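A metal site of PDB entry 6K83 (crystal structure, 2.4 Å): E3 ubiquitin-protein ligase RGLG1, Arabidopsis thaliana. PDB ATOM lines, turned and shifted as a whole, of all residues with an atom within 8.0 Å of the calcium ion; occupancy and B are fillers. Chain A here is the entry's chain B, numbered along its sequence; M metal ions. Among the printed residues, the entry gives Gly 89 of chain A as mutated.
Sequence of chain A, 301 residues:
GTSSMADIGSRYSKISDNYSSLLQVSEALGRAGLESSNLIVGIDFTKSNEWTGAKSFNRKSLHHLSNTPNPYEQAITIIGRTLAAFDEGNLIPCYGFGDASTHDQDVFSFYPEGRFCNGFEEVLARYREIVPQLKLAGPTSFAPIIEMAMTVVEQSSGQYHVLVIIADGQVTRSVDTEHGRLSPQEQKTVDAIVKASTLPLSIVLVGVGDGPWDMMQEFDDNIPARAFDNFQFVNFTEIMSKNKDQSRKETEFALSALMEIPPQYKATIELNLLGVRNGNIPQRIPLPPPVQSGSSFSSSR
N of Leu 39 lies close to OD2 of Asp 87 (2.8 Å).
The backbone NH of Asn 38 is in hydrogen-bond range of the backbone carbonyl oxygen of Phe 86, 3.3 Å away.
OE2 of Glu 88 is in hydrogen-bond range of ND2 of Asn 38, 3.3 Å away.
OD1 of Asp 87 lies close to N of Asn 90 (3.1 Å).
Three residues have an atom within 4 Å of the calcium ion: Asn 38, Asp 87 and Leu 91.
The calcium ion is bound by the backbone carbonyl oxygen (O) of Leu 91 (2.4 Å), the side-chain amide oxygen (OD1) of Asn 38 (2.5 Å), the side-chain carboxylate (OD2) of Asp 87 (2.6 Å) and the side-chain carboxylate (OD1) of Asp 87 (2.6 Å).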
ATOM      1  N   SER A  37      26.735  -0.556 -11.423  1.00  0.00           N
ATOM      2  CA  SER A  37      27.585  -1.123 -10.382  1.00  0.00           C
ATOM      3  C   SER A  37      26.741  -1.608  -9.223  1.00  0.00           C
ATOM      4  O   SER A  37      25.600  -1.187  -9.047  1.00  0.00           O
ATOM      5  CB  SER A  37      28.618  -0.108  -9.895  1.00  0.00           C
ATOM      6  OG  SER A  37      28.090   0.728  -8.873  1.00  0.00           O
ATOM      7  N   ASN A  38      27.321  -2.494  -8.428  1.00  0.00           N
ATOM      8  CA  ASN A  38      26.677  -3.010  -7.234  1.00  0.00           C
ATOM      9  C   ASN A  38      27.639  -3.011  -6.063  1.00  0.00           C
ATOM     10  O   ASN A  38      28.857  -2.936  -6.239  1.00  0.00           O
ATOM     11  CB  ASN A  38      26.128  -4.410  -7.515  1.00  0.00           C
ATOM     12  CG  ASN A  38      24.887  -4.378  -8.392  1.00  0.00           C
ATOM     13  OD1 ASN A  38      23.777  -4.264  -7.877  1.00  0.00           O
ATOM     14  ND2 ASN A  38      25.072  -4.471  -9.702  1.00  0.00           N
ATOM     15  N   LEU A  39      27.103  -3.078  -4.849  1.00  0.00           N
ATOM     16  CA  LEU A  39      27.944  -3.117  -3.668  1.00  0.00           C
ATOM     17  C   LEU A  39      27.818  -4.455  -2.944  1.00  0.00           C
ATOM     18  O   LEU A  39      26.783  -5.097  -3.034  1.00  0.00           O
ATOM     19  CB  LEU A  39      27.593  -1.958  -2.728  1.00  0.00           C
ATOM     20  CG  LEU A  39      27.904  -0.567  -3.284  1.00  0.00           C
ATOM     21  CD1 LEU A  39      27.496   0.465  -2.261  1.00  0.00           C
ATOM     22  CD2 LEU A  39      29.375  -0.423  -3.635  1.00  0.00           C
ATOM     23  N   ILE A  40      28.890  -4.874  -2.265  1.00  0.00           N
ATOM     24  CA  ILE A  40      28.865  -5.994  -1.330  1.00  0.00           C
ATOM     25  C   ILE A  40      29.509  -5.571   0.007  1.00  0.00           C
ATOM     26  O   ILE A  40      30.593  -4.978   0.016  1.00  0.00           O
ATOM     27  CB  ILE A  40      29.602  -7.241  -1.852  1.00  0.00           C
ATOM     28  CG1 ILE A  40      29.298  -7.460  -3.333  1.00  0.00           C
ATOM     29  CG2 ILE A  40      29.244  -8.460  -1.024  1.00  0.00           C
ATOM     30  CD1 ILE A  40      30.216  -8.452  -3.989  1.00  0.00           C
ATOM     31  N   PHE A  86      26.032   3.796  -5.873  1.00  0.00           N
ATOM     32  CA  PHE A  86      26.843   2.768  -6.539  1.00  0.00           C
ATOM     33  C   PHE A  86      26.284   1.350  -6.407  1.00  0.00           C
ATOM     34  O   PHE A  86      26.887   0.386  -6.871  1.00  0.00           O
ATOM     35  CB  PHE A  86      28.299   2.831  -6.020  1.00  0.00           C
ATOM     36  CG  PHE A  86      29.089   3.978  -6.587  1.00  0.00           C
ATOM     37  CD1 PHE A  86      29.006   5.236  -6.041  1.00  0.00           C
ATOM     38  CD2 PHE A  86      29.892   3.788  -7.703  1.00  0.00           C
ATOM     39  CE1 PHE A  86      29.715   6.306  -6.585  1.00  0.00           C
ATOM     40  CE2 PHE A  86      30.607   4.844  -8.255  1.00  0.00           C
ATOM     41  CZ  PHE A  86      30.522   6.102  -7.685  1.00  0.00           C
ATOM     42  N   ASP A  87      25.123   1.237  -5.766  1.00  0.00           N
ATOM     43  CA  ASP A  87      24.380  -0.021  -5.817  1.00  0.00           C
ATOM     44  C   ASP A  87      23.076   0.253  -6.531  1.00  0.00           C
ATOM     45  O   ASP A  87      22.227   0.956  -5.995  1.00  0.00           O
ATOM     46  CB  ASP A  87      24.119  -0.583  -4.423  1.00  0.00           C
ATOM     47  CG  ASP A  87      23.553  -1.986  -4.472  1.00  0.00           C
ATOM     48  OD1 ASP A  87      22.338  -2.137  -4.746  1.00  0.00           O
ATOM     49  OD2 ASP A  87      24.336  -2.947  -4.260  1.00  0.00           O
ATOM     50  N   GLU A  88      22.918  -0.292  -7.735  1.00  0.00           N
ATOM     51  CA  GLU A  88      21.897   0.223  -8.656  1.00  0.00           C
ATOM     52  C   GLU A  88      20.494  -0.065  -8.162  1.00  0.00           C
ATOM     53  O   GLU A  88      19.578   0.743  -8.400  1.00  0.00           O
ATOM     54  CB  GLU A  88      22.078  -0.360 -10.070  1.00  0.00           C
ATOM     55  CG  GLU A  88      21.853  -1.859 -10.173  1.00  0.00           C
ATOM     56  CD  GLU A  88      22.317  -2.378 -11.513  1.00  0.00           C
ATOM     57  OE1 GLU A  88      22.422  -1.523 -12.421  1.00  0.00           O
ATOM     58  OE2 GLU A  88      22.587  -3.598 -11.661  1.00  0.00           O
ATOM     59  N   GLY A  89      20.321  -1.186  -7.469  1.00  0.00           N
ATOM     60  CA  GLY A  89      19.013  -1.568  -6.961  1.00  0.00           C
ATOM     61  C   GLY A  89      18.750  -1.339  -5.480  1.00  0.00           C
ATOM     62  O   GLY A  89      17.722  -1.799  -4.961  1.00  0.00           O
ATOM     63  N   ASN A  90      19.648  -0.638  -4.792  1.00  0.00           N
ATOM     64  CA  ASN A  90      19.591  -0.486  -3.327  1.00  0.00           C
ATOM     65  C   ASN A  90      19.387  -1.824  -2.581  1.00  0.00           C
ATOM     66  O   ASN A  90      18.832  -1.860  -1.467  1.00  0.00           O
ATOM     67  CB  ASN A  90      18.486   0.508  -2.934  1.00  0.00           C
ATOM     68  CG  ASN A  90      18.778   1.216  -1.613  1.00  0.00           C
ATOM     69  OD1 ASN A  90      19.936   1.473  -1.280  1.00  0.00           O
ATOM     70  ND2 ASN A  90      17.721   1.529  -0.857  1.00  0.00           N
ATOM     71  N   LEU A  91      19.840  -2.911  -3.197  1.00  0.00           N
ATOM     72  CA  LEU A  91      19.795  -4.249  -2.613  1.00  0.00           C
ATOM     73  C   LEU A  91      21.218  -4.797  -2.438  1.00  0.00           C
ATOM     74  O   LEU A  91      21.887  -5.072  -3.435  1.00  0.00           O
ATOM     75  CB  LEU A  91      18.974  -5.200  -3.479  1.00  0.00           C
ATOM     76  CG  LEU A  91      17.556  -5.531  -3.007  1.00  0.00           C
ATOM     77  CD1 LEU A  91      16.954  -6.639  -3.871  1.00  0.00           C
ATOM     78  CD2 LEU A  91      17.590  -5.954  -1.542  1.00  0.00           C
ATOM     79  N   ILE A  92      21.657  -4.978  -1.198  1.00  0.00           N
ATOM     80  CA  ILE A  92      23.058  -5.255  -0.914  1.00  0.00           C
ATOM     81  C   ILE A  92      23.294  -6.580  -0.173  1.00  0.00           C
ATOM     82  O   ILE A  92      22.863  -6.742   0.958  1.00  0.00           O
ATOM     83  CB  ILE A  92      23.684  -4.110  -0.089  1.00  0.00           C
ATOM     84  CG1 ILE A  92      23.513  -2.774  -0.804  1.00  0.00           C
ATOM     85  CG2 ILE A  92      25.155  -4.367   0.168  1.00  0.00           C
ATOM     86  CD1 ILE A  92      22.403  -1.929  -0.257  1.00  0.00           C
ATOM     87  N   PRO A  93      23.970  -7.525  -0.808  1.00  0.00           N
ATOM     88  CA  PRO A  93      24.415  -8.655   0.003  1.00  0.00           C
ATOM     89  C   PRO A  93      25.347  -8.192   1.128  1.00  0.00           C
ATOM     90  O   PRO A  93      26.235  -7.350   0.907  1.00  0.00           O
ATOM     91  CB  PRO A  93      25.142  -9.581  -0.992  1.00  0.00           C
ATOM     92  CG  PRO A  93      25.289  -8.786  -2.244  1.00  0.00           C
ATOM     93  CD  PRO A  93      24.233  -7.722  -2.245  1.00  0.00           C
ATOM     94  N   PHE A 116      18.736 -10.183   0.646  1.00  0.00           N
ATOM     95  CA  PHE A 116      19.644  -9.041   0.763  1.00  0.00           C
ATOM     96  C   PHE A 116      19.044  -7.901   1.582  1.00  0.00           C
ATOM     97  O   PHE A 116      17.853  -7.886   1.883  1.00  0.00           O
ATOM     98  CB  PHE A 116      20.040  -8.531  -0.618  1.00  0.00           C
ATOM     99  CG  PHE A 116      20.828  -9.509  -1.438  1.00  0.00           C
ATOM    100  CD1 PHE A 116      21.319 -10.678  -0.877  1.00  0.00           C
ATOM    101  CD2 PHE A 116      21.100  -9.240  -2.774  1.00  0.00           C
ATOM    102  CE1 PHE A 116      22.051 -11.588  -1.646  1.00  0.00           C
ATOM    103  CE2 PHE A 116      21.836 -10.127  -3.543  1.00  0.00           C
ATOM    104  CZ  PHE A 116      22.305 -11.306  -2.980  1.00  0.00           C
ATOM    105  N   CYS A 117      19.885  -6.934   1.937  1.00  0.00           N
ATOM    106  CA  CYS A 117      19.450  -5.787   2.730  1.00  0.00           C
ATOM    107  C   CYS A 117      18.780  -4.744   1.843  1.00  0.00           C
ATOM    108  O   CYS A 117      19.257  -4.426   0.763  1.00  0.00           O
ATOM    109  CB  CYS A 117      20.632  -5.163   3.474  1.00  0.00           C
ATOM    110  SG  CYS A 117      21.239  -6.142   4.925  1.00  0.00           S
ATOM    111  N   HIS A 161      31.321  -5.181  -9.447  1.00  0.00           N
ATOM    112  CA  HIS A 161      30.988  -4.972  -8.033  1.00  0.00           C
ATOM    113  C   HIS A 161      32.106  -4.273  -7.296  1.00  0.00           C
ATOM    114  O   HIS A 161      33.273  -4.425  -7.630  1.00  0.00           O
ATOM    115  CB  HIS A 161      30.711  -6.310  -7.314  1.00  0.00           C
ATOM    116  CG  HIS A 161      29.441  -6.987  -7.725  1.00  0.00           C
ATOM    117  ND1 HIS A 161      29.273  -7.581  -8.963  1.00  0.00           N
ATOM    118  CD2 HIS A 161      28.297  -7.231  -7.032  1.00  0.00           C
ATOM    119  CE1 HIS A 161      28.071  -8.149  -9.016  1.00  0.00           C
ATOM    120  NE2 HIS A 161      27.466  -7.944  -7.861  1.00  0.00           N
HETATM  121 CA    CA M   1      22.834  -4.594  -5.532  1.00  0.00          CA
